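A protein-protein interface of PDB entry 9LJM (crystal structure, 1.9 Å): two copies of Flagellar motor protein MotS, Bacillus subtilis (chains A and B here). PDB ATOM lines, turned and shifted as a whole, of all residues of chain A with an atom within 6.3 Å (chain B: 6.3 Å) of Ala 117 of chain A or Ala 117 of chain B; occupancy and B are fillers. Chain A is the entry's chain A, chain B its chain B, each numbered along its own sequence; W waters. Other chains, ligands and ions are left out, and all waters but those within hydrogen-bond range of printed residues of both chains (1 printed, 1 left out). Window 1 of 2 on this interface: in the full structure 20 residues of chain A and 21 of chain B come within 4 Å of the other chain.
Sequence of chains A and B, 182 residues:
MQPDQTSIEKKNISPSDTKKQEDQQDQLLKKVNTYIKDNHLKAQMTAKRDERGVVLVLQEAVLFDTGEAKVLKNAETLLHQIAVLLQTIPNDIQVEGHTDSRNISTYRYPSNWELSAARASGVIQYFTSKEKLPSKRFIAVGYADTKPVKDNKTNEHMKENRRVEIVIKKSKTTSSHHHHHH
Of the 18 printed residues of chain B, 8 touch a printed residue of chain A.
Hydrophobic or aromatic side chains of chain B within 4 Å of the printed part of chain A: Ala 117, Ala 140 and Val 141.
Printed residues of chain A that touch a printed residue of chain B: Trp 113, Glu 114, Ala 117, Ala 118, Ser 121, Ala 140, Val 141 and Gly 142.
Hydrophobic or aromatic side chains of chain A that line the printed part of chain B: Trp 113, Ala 117, Ala 118, Ala 140 and Val 141.
Among the printed residues, 14 pairs touch across the chains.
Among the printed residues, no Asp or Glu carboxylate lies within 4 Å of a Lys or Arg side-chain nitrogen of the other chain.
Trp 113 of chain A touches Ser 121 of chain B, and with the chains exchanged Ser 121 of chain A touches Trp 113 of chain B.
Glu 114 of chain A touches Ser 121 of chain B, and with the chains exchanged Ser 121 of chain A touches Glu 114 of chain B.
Ala 117 of chain A touches Ser 121 of chain B, and with the chains exchanged Ser 121 of chain A touches Ala 117 of chain B.
Ala 140 of chain A touches Gly 142 of chain B, and with the chains exchanged Gly 142 of chain A touches Ala 140 of chain B.
Of the 14 pairs that touch across the chains among the printed residues, 12 have their exchanged pair printed and touching as well.
The backbone carbonyl oxygen (O) of Val 141 of chain A lies within hydrogen-bond range of the backbone NH (N) of Gly 97 of chain A, 2.8 Å away.
The backbone carbonyl oxygen of Trp 113 of chain A lies within hydrogen-bond range of the side-chain hydroxyl of Ser 116 of chain A (3.0 Å).
O of Ala 117 of chain A is in hydrogen-bond range of OG of Ser 121 of chain A, 2.9 Å away.
The backbone NH of Gly 97 of chain B sits at hydrogen-bond distance from the backbone carbonyl oxygen of Val 141 of chain B (2.8 Å).
OG of Ser 116 of chain B lies within hydrogen-bond range of O of Trp 113 of chain B, 3.0 Å away.
O of Ala 117 of chain B lies within hydrogen-bond range of OG of Ser 121 of chain B (2.9 Å).
Ala 117 of chain A touches just these residues of chain B: Ala 117 (3.7 Å) and Ser 121 (3.5 Å).
Of chain A, only Ala 117 and Ser 121 come within 4 Å of Ala 117 of chain B.
Of the printed residues of chain A, Val 141 of chain B touches Ala 140.
Of the printed residues of chain A, Gly 122 of chain B touches Glu 114 (3.5 Å).
Of the printed residues of chain B, Gly 142 of chain A touches Ala 140.
Printed residues of chain B within 4 Å of Ser 121 of chain A: Trp 113, Glu 114 and Ala 117.
Printed residues of chain A within 4 Å of Trp 113 of chain B: Ser 121.
The nearest printed residue of chain B that does not touch Ala 140 of chain A is Trp 113 of chain B (4.05 Å).
Water W1 bridges the backbone carbonyl oxygen of Ala 118 of chain A (2.9 Å) and the side-chain carboxylate of Glu 114 of chain B (2.9 Å).
The backbone carbonyl oxygen (O) of Trp 113 of chain A is in hydrogen-bond range of the side-chain hydroxyl (OG) of Ser 121 of chain B (3.1 Å).
The side-chain hydroxyl (OG) of Ser 121 of chain A sits at hydrogen-bond distance from the backbone carbonyl oxygen (O) of Trp 113 of chain B, at 3.1 Å.
The backbone carbonyl oxygen (O) of Ala 140 of chain A is in hydrogen-bond range of the backbone NH (N) of Gly 142 of chain B (2.8 Å).
The backbone NH (N) of Gly 142 of chain A lies within hydrogen-bond range of the backbone carbonyl oxygen (O) of Ala 140 of chain B (2.8 Å).
Among the printed residues, pairs that only touch across the chains: Ala 140 of chain A with Val 141 of chain B (3.3 Å), Val 141 of chain A with Ala 140 of chain B (3.3 Å), Ala 118 of chain A with Glu 114 of chain B (3.3 Å), Ser 121 of chain A with Ala 117 of chain B (3.4 Å), Ala 117 of chain A with Ser 121 of chain B (3.5 Å), Glu 114 of chain A with Gly 122 of chain B (3.5 Å), Glu 114 of chain A with Ser 121 of chain B (3.6 Å), Ala 117 of chain A with Ala 117 of chain B (3.7 Å), Ser 121 of chain A with Glu 114 of chain B (3.7 Å) and Ala 140 of chain A with Ala 140 of chain B (3.9 Å).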
ATOM      1  N   GLY A  97      -4.931 -20.106  25.816  1.00  0.00           N
ATOM      2  CA  GLY A  97      -5.465 -21.282  26.486  1.00  0.00           C
ATOM      3  C   GLY A  97      -4.339 -22.174  26.980  1.00  0.00           C
ATOM      4  O   GLY A  97      -3.308 -22.312  26.320  1.00  0.00           O
ATOM      5  N   HIS A  98      -4.551 -22.778  28.151  1.00  0.00           N
ATOM      6  CA  HIS A  98      -3.572 -23.662  28.768  1.00  0.00           C
ATOM      7  C   HIS A  98      -4.282 -24.888  29.323  1.00  0.00           C
ATOM      8  O   HIS A  98      -5.423 -24.806  29.788  1.00  0.00           O
ATOM      9  CB  HIS A  98      -2.813 -22.979  29.914  1.00  0.00           C
ATOM     10  CG  HIS A  98      -2.010 -21.787  29.495  1.00  0.00           C
ATOM     11  ND1 HIS A  98      -0.661 -21.855  29.219  1.00  0.00           N
ATOM     12  CD2 HIS A  98      -2.365 -20.493  29.321  1.00  0.00           C
ATOM     13  CE1 HIS A  98      -0.222 -20.655  28.888  1.00  0.00           C
ATOM     14  NE2 HIS A  98      -1.236 -19.810  28.941  1.00  0.00           N
ATOM     15  N   ASN A 112      -4.231 -31.944  23.938  1.00  0.00           N
ATOM     16  CA  ASN A 112      -4.190 -30.738  24.755  1.00  0.00           C
ATOM     17  C   ASN A 112      -3.915 -29.491  23.924  1.00  0.00           C
ATOM     18  O   ASN A 112      -4.296 -28.391  24.338  1.00  0.00           O
ATOM     19  CB  ASN A 112      -3.134 -30.890  25.849  1.00  0.00           C
ATOM     20  CG  ASN A 112      -3.695 -31.515  27.114  1.00  0.00           C
ATOM     21  OD1 ASN A 112      -4.902 -31.471  27.358  1.00  0.00           O
ATOM     22  ND2 ASN A 112      -2.823 -32.105  27.924  1.00  0.00           N
ATOM     23  N   TRP A 113      -3.271 -29.634  22.765  1.00  0.00           N
ATOM     24  CA  TRP A 113      -3.121 -28.495  21.867  1.00  0.00           C
ATOM     25  C   TRP A 113      -4.486 -28.003  21.406  1.00  0.00           C
ATOM     26  O   TRP A 113      -4.793 -26.809  21.494  1.00  0.00           O
ATOM     27  CB  TRP A 113      -2.249 -28.877  20.669  1.00  0.00           C
ATOM     28  CG  TRP A 113      -0.806 -29.076  21.026  1.00  0.00           C
ATOM     29  CD1 TRP A 113      -0.154 -30.268  21.160  1.00  0.00           C
ATOM     30  CD2 TRP A 113       0.160 -28.057  21.313  1.00  0.00           C
ATOM     31  NE1 TRP A 113       1.158 -30.054  21.506  1.00  0.00           N
ATOM     32  CE2 TRP A 113       1.375 -28.705  21.609  1.00  0.00           C
ATOM     33  CE3 TRP A 113       0.115 -26.659  21.349  1.00  0.00           C
ATOM     34  CZ2 TRP A 113       2.536 -28.005  21.930  1.00  0.00           C
ATOM     35  CZ3 TRP A 113       1.269 -25.966  21.671  1.00  0.00           C
ATOM     36  CH2 TRP A 113       2.462 -26.639  21.958  1.00  0.00           C
ATOM     37  N   GLU A 114      -5.333 -28.923  20.940  1.00  0.00           N
ATOM     38  CA  GLU A 114      -6.664 -28.546  20.470  1.00  0.00           C
ATOM     39  C   GLU A 114      -7.519 -27.997  21.603  1.00  0.00           C
ATOM     40  O   GLU A 114      -8.230 -27.001  21.426  1.00  0.00           O
ATOM     41  CB  GLU A 114      -7.355 -29.743  19.815  1.00  0.00           C
ATOM     42  CG  GLU A 114      -6.795 -30.167  18.465  1.00  0.00           C
ATOM     43  CD  GLU A 114      -5.608 -31.100  18.570  1.00  0.00           C
ATOM     44  OE1 GLU A 114      -5.130 -31.312  19.700  1.00  0.00           O
ATOM     45  OE2 GLU A 114      -5.166 -31.641  17.527  1.00  0.00           O
ATOM     46  N   LEU A 115      -7.466 -28.632  22.777  1.00  0.00           N
ATOM     47  CA  LEU A 115      -8.286 -28.167  23.894  1.00  0.00           C
ATOM     48  C   LEU A 115      -7.894 -26.757  24.318  1.00  0.00           C
ATOM     49  O   LEU A 115      -8.759 -25.896  24.521  1.00  0.00           O
ATOM     50  CB  LEU A 115      -8.170 -29.120  25.082  1.00  0.00           C
ATOM     51  CG  LEU A 115      -9.019 -28.739  26.301  1.00  0.00           C
ATOM     52  CD1 LEU A 115     -10.495 -28.795  25.940  1.00  0.00           C
ATOM     53  CD2 LEU A 115      -8.725 -29.632  27.502  1.00  0.00           C
ATOM     54  N   SER A 116      -6.590 -26.504  24.470  1.00  0.00           N
ATOM     55  CA  SER A 116      -6.153 -25.178  24.891  1.00  0.00           C
ATOM     56  C   SER A 116      -6.531 -24.126  23.857  1.00  0.00           C
ATOM     57  O   SER A 116      -6.960 -23.023  24.211  1.00  0.00           O
ATOM     58  CB  SER A 116      -4.646 -25.170  25.152  1.00  0.00           C
ATOM     59  OG  SER A 116      -3.898 -25.259  23.948  1.00  0.00           O
ATOM     60  N   ALA A 117      -6.403 -24.463  22.571  1.00  0.00           N
ATOM     61  CA  ALA A 117      -6.750 -23.516  21.519  1.00  0.00           C
ATOM     62  C   ALA A 117      -8.256 -23.344  21.386  1.00  0.00           C
ATOM     63  O   ALA A 117      -8.722 -22.248  21.055  1.00  0.00           O
ATOM     64  CB  ALA A 117      -6.148 -23.965  20.186  1.00  0.00           C
ATOM     65  N   ALA A 118      -9.030 -24.399  21.649  1.00  0.00           N
ATOM     66  CA  ALA A 118     -10.481 -24.273  21.592  1.00  0.00           C
ATOM     67  C   ALA A 118     -11.017 -23.398  22.717  1.00  0.00           C
ATOM     68  O   ALA A 118     -12.063 -22.760  22.558  1.00  0.00           O
ATOM     69  CB  ALA A 118     -11.139 -25.652  21.644  1.00  0.00           C
ATOM     70  N   ARG A 119     -10.325 -23.359  23.858  1.00  0.00           N
ATOM     71  CA  ARG A 119     -10.783 -22.516  24.959  1.00  0.00           C
ATOM     72  C   ARG A 119     -10.496 -21.047  24.683  1.00  0.00           C
ATOM     73  O   ARG A 119     -11.352 -20.186  24.922  1.00  0.00           O
ATOM     74  CB  ARG A 119     -10.133 -22.962  26.264  1.00  0.00           C
ATOM     75  CG  ARG A 119     -10.712 -24.266  26.776  1.00  0.00           C
ATOM     76  CD  ARG A 119     -10.057 -24.741  28.050  1.00  0.00           C
ATOM     77  NE  ARG A 119     -10.893 -25.748  28.693  1.00  0.00           N
ATOM     78  CZ  ARG A 119     -10.762 -26.141  29.952  1.00  0.00           C
ATOM     79  NH1 ARG A 119      -9.817 -25.648  30.735  1.00  0.00           N
ATOM     80  NH2 ARG A 119     -11.606 -27.047  30.438  1.00  0.00           N
ATOM     81  N   ALA A 120      -9.300 -20.738  24.182  1.00  0.00           N
ATOM     82  CA  ALA A 120      -9.022 -19.372  23.755  1.00  0.00           C
ATOM     83  C   ALA A 120      -9.992 -18.940  22.662  1.00  0.00           C
ATOM     84  O   ALA A 120     -10.495 -17.809  22.676  1.00  0.00           O
ATOM     85  CB  ALA A 120      -7.575 -19.259  23.277  1.00  0.00           C
ATOM     86  N   SER A 121     -10.294 -19.846  21.727  1.00  0.00           N
ATOM     87  CA  SER A 121     -11.209 -19.533  20.633  1.00  0.00           C
ATOM     88  C   SER A 121     -12.629 -19.294  21.139  1.00  0.00           C
ATOM     89  O   SER A 121     -13.315 -18.379  20.669  1.00  0.00           O
ATOM     90  CB  SER A 121     -11.197 -20.666  19.607  1.00  0.00           C
ATOM     91  OG  SER A 121      -9.958 -20.714  18.923  1.00  0.00           O
ATOM     92  N   GLY A 122     -13.091 -20.113  22.088  1.00  0.00           N
ATOM     93  CA  GLY A 122     -14.431 -19.927  22.620  1.00  0.00           C
ATOM     94  C   GLY A 122     -14.596 -18.595  23.326  1.00  0.00           C
ATOM     95  O   GLY A 122     -15.662 -17.976  23.267  1.00  0.00           O
ATOM     96  N   ALA A 140      -6.110 -16.000  18.819  1.00  0.00           N
ATOM     97  CA  ALA A 140      -6.269 -17.163  19.688  1.00  0.00           C
ATOM     98  C   ALA A 140      -4.956 -17.934  19.750  1.00  0.00           C
ATOM     99  O   ALA A 140      -4.343 -18.214  18.712  1.00  0.00           O
ATOM    100  CB  ALA A 140      -7.394 -18.071  19.190  1.00  0.00           C
ATOM    101  N   VAL A 141      -4.520 -18.269  20.963  1.00  0.00           N
ATOM    102  CA  VAL A 141      -3.235 -18.927  21.169  1.00  0.00           C
ATOM    103  C   VAL A 141      -3.440 -20.128  22.080  1.00  0.00           C
ATOM    104  O   VAL A 141      -4.089 -20.018  23.126  1.00  0.00           O
ATOM    105  CB  VAL A 141      -2.187 -17.969  21.768  1.00  0.00           C
ATOM    106  CG1 VAL A 141      -0.838 -18.664  21.879  1.00  0.00           C
ATOM    107  CG2 VAL A 141      -2.080 -16.689  20.940  1.00  0.00           C
ATOM    108  N   GLY A 142      -2.887 -21.271  21.681  1.00  0.00           N
ATOM    109  CA  GLY A 142      -2.939 -22.469  22.496  1.00  0.00           C
ATOM    110  C   GLY A 142      -1.555 -22.939  22.892  1.00  0.00           C
ATOM    111  O   GLY A 142      -0.675 -23.088  22.036  1.00  0.00           O
ATOM    112  N   TYR A 143      -1.343 -23.171  24.184  1.00  0.00           N
ATOM    113  CA  TYR A 143      -0.041 -23.586  24.687  1.00  0.00           C
ATOM    114  C   TYR A 143       0.001 -25.041  25.133  1.00  0.00           C
ATOM    115  O   TYR A 143       1.078 -25.527  25.496  1.00  0.00           O
ATOM    116  CB  TYR A 143       0.392 -22.683  25.850  1.00  0.00           C
ATOM    117  CG  TYR A 143       0.796 -21.285  25.425  1.00  0.00           C
ATOM    118  CD1 TYR A 143       2.069 -21.030  24.926  1.00  0.00           C
ATOM    119  CD2 TYR A 143      -0.091 -20.222  25.532  1.00  0.00           C
ATOM    120  CE1 TYR A 143       2.448 -19.752  24.539  1.00  0.00           C
ATOM    121  CE2 TYR A 143       0.280 -18.941  25.152  1.00  0.00           C
ATOM    122  CZ  TYR A 143       1.547 -18.711  24.656  1.00  0.00           C
ATOM    123  OH  TYR A 143       1.911 -17.439  24.276  1.00  0.00           O
ATOM    124  N   ALA A 144      -1.124 -25.751  25.094  1.00  0.00           N
ATOM    125  CA  ALA A 144      -1.228 -27.108  25.649  1.00  0.00           C
ATOM    126  C   ALA A 144      -0.696 -27.041  27.081  1.00  0.00           C
ATOM    127  O   ALA A 144      -1.102 -26.143  27.833  1.00  0.00           O
ATOM    128  CB  ALA A 144      -0.527 -28.103  24.735  1.00  0.00           C
ATOM    129  N   GLY B  97      -3.171 -20.965  11.950  1.00  0.00           N
ATOM    130  CA  GLY B  97      -4.314 -21.392  11.161  1.00  0.00           C
ATOM    131  C   GLY B  97      -5.091 -20.185  10.663  1.00  0.00           C
ATOM    132  O   GLY B  97      -5.231 -19.189  11.371  1.00  0.00           O
ATOM    133  N   HIS B  98      -5.583 -20.287   9.430  1.00  0.00           N
ATOM    134  CA  HIS B  98      -6.326 -19.212   8.789  1.00  0.00           C
ATOM    135  C   HIS B  98      -7.523 -19.803   8.059  1.00  0.00           C
ATOM    136  O   HIS B  98      -7.409 -20.851   7.420  1.00  0.00           O
ATOM    137  CB  HIS B  98      -5.460 -18.434   7.780  1.00  0.00           C
ATOM    138  CG  HIS B  98      -4.263 -17.769   8.385  1.00  0.00           C
ATOM    139  ND1 HIS B  98      -4.286 -16.474   8.857  1.00  0.00           N
ATOM    140  CD2 HIS B  98      -2.994 -18.209   8.559  1.00  0.00           C
ATOM    141  CE1 HIS B  98      -3.090 -16.154   9.318  1.00  0.00           C
ATOM    142  NE2 HIS B  98      -2.286 -17.187   9.144  1.00  0.00           N
ATOM    143  N   ASN B 112     -14.997 -19.919  12.970  1.00  0.00           N
ATOM    144  CA  ASN B 112     -13.718 -19.931  12.263  1.00  0.00           C
ATOM    145  C   ASN B 112     -12.533 -19.751  13.204  1.00  0.00           C
ATOM    146  O   ASN B 112     -11.428 -20.205  12.892  1.00  0.00           O
ATOM    147  CB  ASN B 112     -13.704 -18.853  11.180  1.00  0.00           C
ATOM    148  CG  ASN B 112     -14.455 -19.275   9.932  1.00  0.00           C
ATOM    149  OD1 ASN B 112     -14.411 -20.438   9.538  1.00  0.00           O
ATOM    150  ND2 ASN B 112     -15.123 -18.325   9.288  1.00  0.00           N
ATOM    151  N   TRP B 113     -12.731 -19.085  14.344  1.00  0.00           N
ATOM    152  CA  TRP B 113     -11.674 -19.037  15.350  1.00  0.00           C
ATOM    153  C   TRP B 113     -11.286 -20.448  15.766  1.00  0.00           C
ATOM    154  O   TRP B 113     -10.103 -20.808  15.797  1.00  0.00           O
ATOM    155  CB  TRP B 113     -12.145 -18.238  16.567  1.00  0.00           C
ATOM    156  CG  TRP B 113     -12.212 -16.771  16.327  1.00  0.00           C
ATOM    157  CD1 TRP B 113     -13.340 -16.024  16.146  1.00  0.00           C
ATOM    158  CD2 TRP B 113     -11.108 -15.870  16.205  1.00  0.00           C
ATOM    159  NE1 TRP B 113     -13.006 -14.708  15.940  1.00  0.00           N
ATOM    160  CE2 TRP B 113     -11.642 -14.587  15.967  1.00  0.00           C
ATOM    161  CE3 TRP B 113      -9.720 -16.020  16.283  1.00  0.00           C
ATOM    162  CZ2 TRP B 113     -10.837 -13.463  15.807  1.00  0.00           C
ATOM    163  CZ3 TRP B 113      -8.922 -14.901  16.126  1.00  0.00           C
ATOM    164  CH2 TRP B 113      -9.483 -13.639  15.889  1.00  0.00           C
ATOM    165  N   GLU B 114     -12.294 -21.269  16.058  1.00  0.00           N
ATOM    166  CA  GLU B 114     -12.067 -22.642  16.496  1.00  0.00           C
ATOM    167  C   GLU B 114     -11.440 -23.480  15.386  1.00  0.00           C
ATOM    168  O   GLU B 114     -10.493 -24.240  15.621  1.00  0.00           O
ATOM    169  CB  GLU B 114     -13.390 -23.262  16.942  1.00  0.00           C
ATOM    170  CG  GLU B 114     -13.390 -24.780  16.978  1.00  0.00           C
ATOM    171  CD  GLU B 114     -12.931 -25.341  18.303  1.00  0.00           C
ATOM    172  OE1 GLU B 114     -13.750 -25.365  19.251  1.00  0.00           O
ATOM    173  OE2 GLU B 114     -11.762 -25.755  18.404  1.00  0.00           O
ATOM    174  N   LEU B 115     -11.975 -23.368  14.169  1.00  0.00           N
ATOM    175  CA  LEU B 115     -11.460 -24.166  13.061  1.00  0.00           C
ATOM    176  C   LEU B 115     -10.005 -23.823  12.763  1.00  0.00           C
ATOM    177  O   LEU B 115      -9.170 -24.719  12.589  1.00  0.00           O
ATOM    178  CB  LEU B 115     -12.330 -23.966  11.820  1.00  0.00           C
ATOM    179  CG  LEU B 115     -11.836 -24.669  10.554  1.00  0.00           C
ATOM    180  CD1 LEU B 115     -11.838 -26.178  10.739  1.00  0.00           C
ATOM    181  CD2 LEU B 115     -12.685 -24.269   9.356  1.00  0.00           C
ATOM    182  N   SER B 116      -9.681 -22.528  12.700  1.00  0.00           N
ATOM    183  CA  SER B 116      -8.306 -22.133  12.413  1.00  0.00           C
ATOM    184  C   SER B 116      -7.360 -22.601  13.511  1.00  0.00           C
ATOM    185  O   SER B 116      -6.258 -23.087  13.228  1.00  0.00           O
ATOM    186  CB  SER B 116      -8.215 -20.615  12.231  1.00  0.00           C
ATOM    187  OG  SER B 116      -8.461 -19.921  13.443  1.00  0.00           O
ATOM    188  N   ALA B 117      -7.785 -22.485  14.770  1.00  0.00           N
ATOM    189  CA  ALA B 117      -6.935 -22.898  15.881  1.00  0.00           C
ATOM    190  C   ALA B 117      -6.777 -24.413  15.926  1.00  0.00           C
ATOM    191  O   ALA B 117      -5.700 -24.921  16.258  1.00  0.00           O
ATOM    192  CB  ALA B 117      -7.510 -22.373  17.195  1.00  0.00           C
ATOM    193  N   ALA B 118      -7.839 -25.153  15.599  1.00  0.00           N
ATOM    194  CA  ALA B 118      -7.742 -26.609  15.596  1.00  0.00           C
ATOM    195  C   ALA B 118      -6.834 -27.105  14.480  1.00  0.00           C
ATOM    196  O   ALA B 118      -6.174 -28.141  14.629  1.00  0.00           O
ATOM    197  CB  ALA B 118      -9.131 -27.231  15.463  1.00  0.00           C
ATOM    198  N   ARG B 119      -6.785 -26.384  13.360  1.00  0.00           N
ATOM    199  CA  ARG B 119      -5.911 -26.796  12.270  1.00  0.00           C
ATOM    200  C   ARG B 119      -4.445 -26.591  12.636  1.00  0.00           C
ATOM    201  O   ARG B 119      -3.602 -27.450  12.347  1.00  0.00           O
ATOM    202  CB  ARG B 119      -6.272 -26.037  10.995  1.00  0.00           C
ATOM    203  CG  ARG B 119      -7.318 -26.764  10.169  1.00  0.00           C
ATOM    204  CD  ARG B 119      -8.023 -25.865   9.167  1.00  0.00           C
ATOM    205  NE  ARG B 119      -8.881 -26.662   8.297  1.00  0.00           N
ATOM    206  CZ  ARG B 119      -9.018 -26.472   6.992  1.00  0.00           C
ATOM    207  NH1 ARG B 119      -8.378 -25.499   6.364  1.00  0.00           N
ATOM    208  NH2 ARG B 119      -9.814 -27.282   6.299  1.00  0.00           N
ATOM    209  N   ALA B 120      -4.124 -25.470  13.283  1.00  0.00           N
ATOM    210  CA  ALA B 120      -2.768 -25.284  13.790  1.00  0.00           C
ATOM    211  C   ALA B 120      -2.424 -26.352  14.820  1.00  0.00           C
ATOM    212  O   ALA B 120      -1.310 -26.890  14.821  1.00  0.00           O
ATOM    213  CB  ALA B 120      -2.616 -23.883  14.387  1.00  0.00           C
ATOM    214  N   SER B 121      -3.387 -26.694  15.682  1.00  0.00           N
ATOM    215  CA  SER B 121      -3.159 -27.686  16.730  1.00  0.00           C
ATOM    216  C   SER B 121      -2.930 -29.078  16.153  1.00  0.00           C
ATOM    217  O   SER B 121      -2.089 -29.833  16.655  1.00  0.00           O
ATOM    218  CB  SER B 121      -4.349 -27.705  17.687  1.00  0.00           C
ATOM    219  OG  SER B 121      -4.456 -26.489  18.391  1.00  0.00           O
ATOM    220  N   GLY B 122      -3.685 -29.446  15.117  1.00  0.00           N
ATOM    221  CA  GLY B 122      -3.504 -30.760  14.519  1.00  0.00           C
ATOM    222  C   GLY B 122      -2.128 -30.931  13.903  1.00  0.00           C
ATOM    223  O   GLY B 122      -1.534 -32.009  13.975  1.00  0.00           O
ATOM    224  N   ALA B 140       0.399 -22.876  19.125  1.00  0.00           N
ATOM    225  CA  ALA B 140      -0.672 -22.925  18.141  1.00  0.00           C
ATOM    226  C   ALA B 140      -1.382 -21.581  18.112  1.00  0.00           C
ATOM    227  O   ALA B 140      -1.703 -21.021  19.166  1.00  0.00           O
ATOM    228  CB  ALA B 140      -1.664 -24.037  18.476  1.00  0.00           C
ATOM    229  N   VAL B 141      -1.626 -21.062  16.913  1.00  0.00           N
ATOM    230  CA  VAL B 141      -2.196 -19.731  16.777  1.00  0.00           C
ATOM    231  C   VAL B 141      -3.337 -19.786  15.769  1.00  0.00           C
ATOM    232  O   VAL B 141      -3.175 -20.327  14.669  1.00  0.00           O
ATOM    233  CB  VAL B 141      -1.134 -18.704  16.343  1.00  0.00           C
ATOM    234  CG1 VAL B 141      -1.780 -17.369  16.105  1.00  0.00           C
ATOM    235  CG2 VAL B 141      -0.008 -18.600  17.374  1.00  0.00           C
ATOM    236  N   GLY B 142      -4.491 -19.246  16.151  1.00  0.00           N
ATOM    237  CA  GLY B 142      -5.629 -19.165  15.251  1.00  0.00           C
ATOM    238  C   GLY B 142      -5.999 -17.731  14.919  1.00  0.00           C
ATOM    239  O   GLY B 142      -6.192 -16.915  15.826  1.00  0.00           O
ATOM    240  N   TYR B 143      -6.101 -17.402  13.629  1.00  0.00           N
ATOM    241  CA  TYR B 143      -6.427 -16.045  13.207  1.00  0.00           C
ATOM    242  C   TYR B 143      -7.832 -15.892  12.645  1.00  0.00           C
ATOM    243  O   TYR B 143      -8.227 -14.764  12.323  1.00  0.00           O
ATOM    244  CB  TYR B 143      -5.424 -15.543  12.159  1.00  0.00           C
ATOM    245  CG  TYR B 143      -4.075 -15.182  12.722  1.00  0.00           C
ATOM    246  CD1 TYR B 143      -3.826 -13.897  13.188  1.00  0.00           C
ATOM    247  CD2 TYR B 143      -3.042 -16.107  12.764  1.00  0.00           C
ATOM    248  CE1 TYR B 143      -2.596 -13.549  13.700  1.00  0.00           C
ATOM    249  CE2 TYR B 143      -1.802 -15.762  13.263  1.00  0.00           C
ATOM    250  CZ  TYR B 143      -1.588 -14.484  13.737  1.00  0.00           C
ATOM    251  OH  TYR B 143      -0.361 -14.138  14.248  1.00  0.00           O
ATOM    252  N   ALA B 144      -8.595 -16.977  12.526  1.00  0.00           N
ATOM    253  CA  ALA B 144      -9.899 -16.960  11.847  1.00  0.00           C
ATOM    254  C   ALA B 144      -9.674 -16.366  10.456  1.00  0.00           C
ATOM    255  O   ALA B 144      -8.715 -16.765   9.778  1.00  0.00           O
ATOM    256  CB  ALA B 144     -10.924 -16.229  12.705  1.00  0.00           C
HETATM  257  O   HOH W   1     -14.502 -23.313  21.149  1.00  0.00           O
